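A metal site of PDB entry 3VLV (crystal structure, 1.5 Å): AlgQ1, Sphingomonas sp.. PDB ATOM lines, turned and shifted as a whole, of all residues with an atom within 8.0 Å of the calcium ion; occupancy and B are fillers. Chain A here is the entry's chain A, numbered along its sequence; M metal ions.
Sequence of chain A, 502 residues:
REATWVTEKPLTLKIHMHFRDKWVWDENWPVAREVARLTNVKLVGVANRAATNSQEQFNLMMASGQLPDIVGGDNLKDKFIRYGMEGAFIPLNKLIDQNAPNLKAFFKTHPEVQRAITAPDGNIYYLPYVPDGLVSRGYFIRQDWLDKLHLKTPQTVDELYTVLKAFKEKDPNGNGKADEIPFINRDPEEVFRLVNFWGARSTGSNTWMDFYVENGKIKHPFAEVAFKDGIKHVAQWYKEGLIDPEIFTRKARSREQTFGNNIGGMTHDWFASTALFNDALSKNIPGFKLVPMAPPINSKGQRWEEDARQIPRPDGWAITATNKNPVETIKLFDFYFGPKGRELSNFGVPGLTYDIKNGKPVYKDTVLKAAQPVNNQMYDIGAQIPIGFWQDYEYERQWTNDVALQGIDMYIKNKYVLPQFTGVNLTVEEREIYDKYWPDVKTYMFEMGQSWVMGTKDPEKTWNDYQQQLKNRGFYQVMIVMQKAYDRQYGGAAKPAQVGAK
OD2 of Asp 171 lies close to N of Gly 174 (3.4 Å).
The side-chain carboxylate (OD1) of Asp 171 lies within hydrogen-bond range of the backbone NH (N) of Gly 176, at 2.9 Å.
ND2 of Asn 173 lies within hydrogen-bond range of O of Asn 262 (3.0 Å).
Six residues have an atom within 4 Å of the calcium ion: Asp 171, Asn 173, Asn 175, Lys 177, Asp 179 and Glu 180.
The nearest printed residue that does not touch the calcium ion is Gly 174 (4.5 Å).
OD2 of Asp 179 is bound to the calcium ion, at 2.3 Å.
O of Lys 177 binds the calcium ion.
OD2 of Asp 171 is bound to the calcium ion.
The side-chain carboxylate (OE1) of Glu 180 is bound to the calcium ion, at 2.3 Å.
OD1 of Asn 173 binds the calcium ion (2.3 Å).
The calcium ion is bound by OD1 of Asn 175, 2.3 Å away.
The side-chain carboxylate (OE2) of Glu 180 binds the calcium ion, at 2.8 Å.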
ATOM      1  N   TRP A 145     -20.389  -5.526  27.479  1.00  0.00           N
ATOM      2  CA  TRP A 145     -19.511  -4.560  26.817  1.00  0.00           C
ATOM      3  C   TRP A 145     -18.658  -5.216  25.732  1.00  0.00           C
ATOM      4  O   TRP A 145     -18.451  -4.628  24.663  1.00  0.00           O
ATOM      5  CB  TRP A 145     -18.628  -3.853  27.856  1.00  0.00           C
ATOM      6  CG  TRP A 145     -19.330  -2.747  28.584  1.00  0.00           C
ATOM      7  CD1 TRP A 145     -20.669  -2.445  28.540  1.00  0.00           C
ATOM      8  CD2 TRP A 145     -18.742  -1.805  29.481  1.00  0.00           C
ATOM      9  NE1 TRP A 145     -20.939  -1.361  29.343  1.00  0.00           N
ATOM     10  CE2 TRP A 145     -19.776  -0.946  29.932  1.00  0.00           C
ATOM     11  CE3 TRP A 145     -17.434  -1.590  29.951  1.00  0.00           C
ATOM     12  CZ2 TRP A 145     -19.540   0.098  30.830  1.00  0.00           C
ATOM     13  CZ3 TRP A 145     -17.205  -0.544  30.842  1.00  0.00           C
ATOM     14  CH2 TRP A 145     -18.253   0.281  31.273  1.00  0.00           C
ATOM     15  N   PHE A 167     -12.719  -0.425  26.025  1.00  0.00           N
ATOM     16  CA  PHE A 167     -13.628  -0.017  27.099  1.00  0.00           C
ATOM     17  C   PHE A 167     -13.455   1.469  27.410  1.00  0.00           C
ATOM     18  O   PHE A 167     -14.435   2.188  27.597  1.00  0.00           O
ATOM     19  CB  PHE A 167     -13.397  -0.833  28.379  1.00  0.00           C
ATOM     20  CG  PHE A 167     -13.919  -2.248  28.329  1.00  0.00           C
ATOM     21  CD1 PHE A 167     -14.613  -2.741  27.225  1.00  0.00           C
ATOM     22  CD2 PHE A 167     -13.745  -3.093  29.427  1.00  0.00           C
ATOM     23  CE1 PHE A 167     -15.087  -4.056  27.201  1.00  0.00           C
ATOM     24  CE2 PHE A 167     -14.232  -4.400  29.419  1.00  0.00           C
ATOM     25  CZ  PHE A 167     -14.898  -4.882  28.301  1.00  0.00           C
ATOM     26  N   LYS A 168     -12.204   1.913  27.458  1.00  0.00           N
ATOM     27  CA  LYS A 168     -11.892   3.303  27.779  1.00  0.00           C
ATOM     28  C   LYS A 168     -12.300   4.272  26.661  1.00  0.00           C
ATOM     29  O   LYS A 168     -12.807   5.361  26.947  1.00  0.00           O
ATOM     30  CB  LYS A 168     -10.397   3.458  28.077  1.00  0.00           C
ATOM     31  CG  LYS A 168     -10.036   4.818  28.653  1.00  0.00           C
ATOM     32  CD  LYS A 168      -8.538   5.053  28.662  1.00  0.00           C
ATOM     33  CE  LYS A 168      -8.214   6.433  29.222  1.00  0.00           C
ATOM     34  NZ  LYS A 168      -8.534   7.527  28.269  1.00  0.00           N
ATOM     35  N   GLU A 169     -12.090   3.874  25.416  1.00  0.00           N
ATOM     36  CA  GLU A 169     -12.162   4.801  24.280  1.00  0.00           C
ATOM     37  C   GLU A 169     -13.430   4.728  23.446  1.00  0.00           C
ATOM     38  O   GLU A 169     -13.795   5.711  22.793  1.00  0.00           O
ATOM     39  CB  GLU A 169     -10.936   4.618  23.376  1.00  0.00           C
ATOM     40  CG  GLU A 169      -9.619   4.975  24.041  1.00  0.00           C
ATOM     41  CD  GLU A 169      -8.405   4.634  23.198  1.00  0.00           C
ATOM     42  OE1 GLU A 169      -8.544   3.910  22.190  1.00  0.00           O
ATOM     43  OE2 GLU A 169      -7.296   5.086  23.554  1.00  0.00           O
ATOM     44  N   LYS A 170     -14.101   3.580  23.460  1.00  0.00           N
ATOM     45  CA  LYS A 170     -15.205   3.333  22.520  1.00  0.00           C
ATOM     46  C   LYS A 170     -16.608   3.421  23.121  1.00  0.00           C
ATOM     47  O   LYS A 170     -17.574   2.894  22.565  1.00  0.00           O
ATOM     48  CB  LYS A 170     -15.010   2.000  21.785  1.00  0.00           C
ATOM     49  CG  LYS A 170     -13.676   1.884  21.029  1.00  0.00           C
ATOM     50  CD  LYS A 170     -13.433   3.056  20.069  1.00  0.00           C
ATOM     51  CE  LYS A 170     -14.321   2.991  18.833  1.00  0.00           C
ATOM     52  NZ  LYS A 170     -13.837   1.964  17.865  1.00  0.00           N
ATOM     53  N   ASP A 171     -16.717   4.109  24.261  1.00  0.00           N
ATOM     54  CA  ASP A 171     -18.014   4.483  24.857  1.00  0.00           C
ATOM     55  C   ASP A 171     -19.027   3.333  24.946  1.00  0.00           C
ATOM     56  O   ASP A 171     -20.129   3.422  24.409  1.00  0.00           O
ATOM     57  CB  ASP A 171     -18.585   5.682  24.079  1.00  0.00           C
ATOM     58  CG  ASP A 171     -19.812   6.286  24.758  1.00  0.00           C
ATOM     59  OD1 ASP A 171     -20.720   6.728  24.024  1.00  0.00           O
ATOM     60  OD2 ASP A 171     -19.864   6.328  25.992  1.00  0.00           O
ATOM     61  N   PRO A 172     -18.657   2.220  25.632  1.00  0.00           N
ATOM     62  CA  PRO A 172     -19.592   1.089  25.713  1.00  0.00           C
ATOM     63  C   PRO A 172     -20.869   1.353  26.508  1.00  0.00           C
ATOM     64  O   PRO A 172     -21.859   0.646  26.305  1.00  0.00           O
ATOM     65  CB  PRO A 172     -18.747  -0.013  26.386  1.00  0.00           C
ATOM     66  CG  PRO A 172     -17.687   0.717  27.115  1.00  0.00           C
ATOM     67  CD  PRO A 172     -17.377   1.912  26.280  1.00  0.00           C
ATOM     68  N   ASN A 173     -20.872   2.343  27.404  1.00  0.00           N
ATOM     69  CA  ASN A 173     -22.115   2.707  28.088  1.00  0.00           C
ATOM     70  C   ASN A 173     -23.000   3.669  27.286  1.00  0.00           C
ATOM     71  O   ASN A 173     -24.135   3.958  27.673  1.00  0.00           O
ATOM     72  CB  ASN A 173     -21.867   3.180  29.546  1.00  0.00           C
ATOM     73  CG  ASN A 173     -21.219   4.556  29.645  1.00  0.00           C
ATOM     74  OD1 ASN A 173     -21.173   5.333  28.683  1.00  0.00           O
ATOM     75  ND2 ASN A 173     -20.724   4.872  30.833  1.00  0.00           N
ATOM     76  N   GLY A 174     -22.461   4.145  26.161  1.00  0.00           N
ATOM     77  CA  GLY A 174     -23.232   4.878  25.147  1.00  0.00           C
ATOM     78  C   GLY A 174     -23.745   6.251  25.519  1.00  0.00           C
ATOM     79  O   GLY A 174     -24.760   6.699  24.993  1.00  0.00           O
ATOM     80  N   ASN A 175     -23.054   6.922  26.435  1.00  0.00           N
ATOM     81  CA  ASN A 175     -23.467   8.258  26.871  1.00  0.00           C
ATOM     82  C   ASN A 175     -22.713   9.412  26.198  1.00  0.00           C
ATOM     83  O   ASN A 175     -22.913  10.581  26.534  1.00  0.00           O
ATOM     84  CB  ASN A 175     -23.440   8.387  28.406  1.00  0.00           C
ATOM     85  CG  ASN A 175     -22.044   8.209  28.995  1.00  0.00           C
ATOM     86  OD1 ASN A 175     -21.042   8.076  28.286  1.00  0.00           O
ATOM     87  ND2 ASN A 175     -21.980   8.204  30.317  1.00  0.00           N
ATOM     88  N   GLY A 176     -21.832   9.067  25.256  1.00  0.00           N
ATOM     89  CA  GLY A 176     -21.047  10.055  24.520  1.00  0.00           C
ATOM     90  C   GLY A 176     -19.902  10.651  25.326  1.00  0.00           C
ATOM     91  O   GLY A 176     -19.253  11.603  24.870  1.00  0.00           O
ATOM     92  N   LYS A 177     -19.650  10.092  26.509  1.00  0.00           N
ATOM     93  CA  LYS A 177     -18.591  10.575  27.390  1.00  0.00           C
ATOM     94  C   LYS A 177     -17.531   9.518  27.624  1.00  0.00           C
ATOM     95  O   LYS A 177     -17.837   8.314  27.675  1.00  0.00           O
ATOM     96  CB  LYS A 177     -19.177  11.031  28.730  1.00  0.00           C
ATOM     97  CG  LYS A 177     -20.199  12.157  28.647  1.00  0.00           C
ATOM     98  CD  LYS A 177     -20.663  12.625  30.019  1.00  0.00           C
ATOM     99  CE  LYS A 177     -21.701  11.675  30.621  1.00  0.00           C
ATOM    100  NZ  LYS A 177     -22.167  12.159  31.953  1.00  0.00           N
ATOM    101  N   ALA A 178     -16.283   9.959  27.765  1.00  0.00           N
ATOM    102  CA  ALA A 178     -15.177   9.084  28.131  1.00  0.00           C
ATOM    103  C   ALA A 178     -15.130   8.968  29.646  1.00  0.00           C
ATOM    104  O   ALA A 178     -14.228   9.507  30.306  1.00  0.00           O
ATOM    105  CB  ALA A 178     -13.863   9.619  27.572  1.00  0.00           C
ATOM    106  N   ASP A 179     -16.112   8.269  30.201  1.00  0.00           N
ATOM    107  CA  ASP A 179     -16.268   8.124  31.651  1.00  0.00           C
ATOM    108  C   ASP A 179     -15.957   6.712  32.138  1.00  0.00           C
ATOM    109  O   ASP A 179     -15.865   6.473  33.343  1.00  0.00           O
ATOM    110  CB  ASP A 179     -17.679   8.561  32.084  1.00  0.00           C
ATOM    111  CG  ASP A 179     -18.797   7.743  31.434  1.00  0.00           C
ATOM    112  OD1 ASP A 179     -19.905   7.730  31.993  1.00  0.00           O
ATOM    113  OD2 ASP A 179     -18.576   7.117  30.360  1.00  0.00           O
ATOM    114  N   GLU A 180     -15.770   5.793  31.200  1.00  0.00           N
ATOM    115  CA  GLU A 180     -15.512   4.394  31.524  1.00  0.00           C
ATOM    116  C   GLU A 180     -14.150   4.203  32.178  1.00  0.00           C
ATOM    117  O   GLU A 180     -13.153   4.816  31.786  1.00  0.00           O
ATOM    118  CB  GLU A 180     -15.603   3.522  30.257  1.00  0.00           C
ATOM    119  CG  GLU A 180     -17.013   3.329  29.724  1.00  0.00           C
ATOM    120  CD  GLU A 180     -17.495   4.450  28.804  1.00  0.00           C
ATOM    121  OE1 GLU A 180     -18.626   4.342  28.294  1.00  0.00           O
ATOM    122  OE2 GLU A 180     -16.751   5.432  28.592  1.00  0.00           O
ATOM    123  N   ILE A 181     -14.139   3.360  33.216  1.00  0.00           N
ATOM    124  CA  ILE A 181     -12.920   2.965  33.901  1.00  0.00           C
ATOM    125  C   ILE A 181     -12.773   1.447  33.726  1.00  0.00           C
ATOM    126  O   ILE A 181     -13.508   0.685  34.356  1.00  0.00           O
ATOM    127  CB  ILE A 181     -12.949   3.331  35.405  1.00  0.00           C
ATOM    128  CG1 ILE A 181     -13.280   4.821  35.598  1.00  0.00           C
ATOM    129  CG2 ILE A 181     -11.629   2.981  36.062  1.00  0.00           C
ATOM    130  CD1 ILE A 181     -13.607   5.220  37.032  1.00  0.00           C
ATOM    131  N   ASN A 261     -22.878   2.951  38.441  1.00  0.00           N
ATOM    132  CA  ASN A 261     -22.931   4.068  37.497  1.00  0.00           C
ATOM    133  C   ASN A 261     -22.576   3.637  36.071  1.00  0.00           C
ATOM    134  O   ASN A 261     -22.499   4.472  35.160  1.00  0.00           O
ATOM    135  CB  ASN A 261     -22.042   5.214  37.963  1.00  0.00           C
ATOM    136  CG  ASN A 261     -22.326   6.525  37.233  1.00  0.00           C
ATOM    137  OD1 ASN A 261     -23.475   6.853  36.939  1.00  0.00           O
ATOM    138  ND2 ASN A 261     -21.272   7.284  36.956  1.00  0.00           N
ATOM    139  N   ASN A 262     -22.374   2.327  35.872  1.00  0.00           N
ATOM    140  CA  ASN A 262     -22.090   1.737  34.557  1.00  0.00           C
ATOM    141  C   ASN A 262     -20.816   2.266  33.906  1.00  0.00           C
ATOM    142  O   ASN A 262     -20.784   2.575  32.712  1.00  0.00           O
ATOM    143  CB  ASN A 262     -23.307   1.890  33.618  1.00  0.00           C
ATOM    144  CG  ASN A 262     -23.273   0.927  32.452  1.00  0.00           C
ATOM    145  OD1 ASN A 262     -22.567  -0.084  32.470  1.00  0.00           O
ATOM    146  ND2 ASN A 262     -24.047   1.234  31.411  1.00  0.00           N
ATOM    147  N   ILE A 263     -19.756   2.367  34.704  1.00  0.00           N
ATOM    148  CA  ILE A 263     -18.456   2.823  34.206  1.00  0.00           C
ATOM    149  C   ILE A 263     -17.339   1.783  34.366  1.00  0.00           C
ATOM    150  O   ILE A 263     -16.325   1.855  33.681  1.00  0.00           O
ATOM    151  CB  ILE A 263     -18.035   4.204  34.795  1.00  0.00           C
ATOM    152  CG1 ILE A 263     -18.044   4.180  36.329  1.00  0.00           C
ATOM    153  CG2 ILE A 263     -18.930   5.315  34.238  1.00  0.00           C
ATOM    154  CD1 ILE A 263     -17.453   5.430  36.976  1.00  0.00           C
HETATM  155 CA    CA M   1     -19.263   6.573  28.220  1.00  0.00          CA
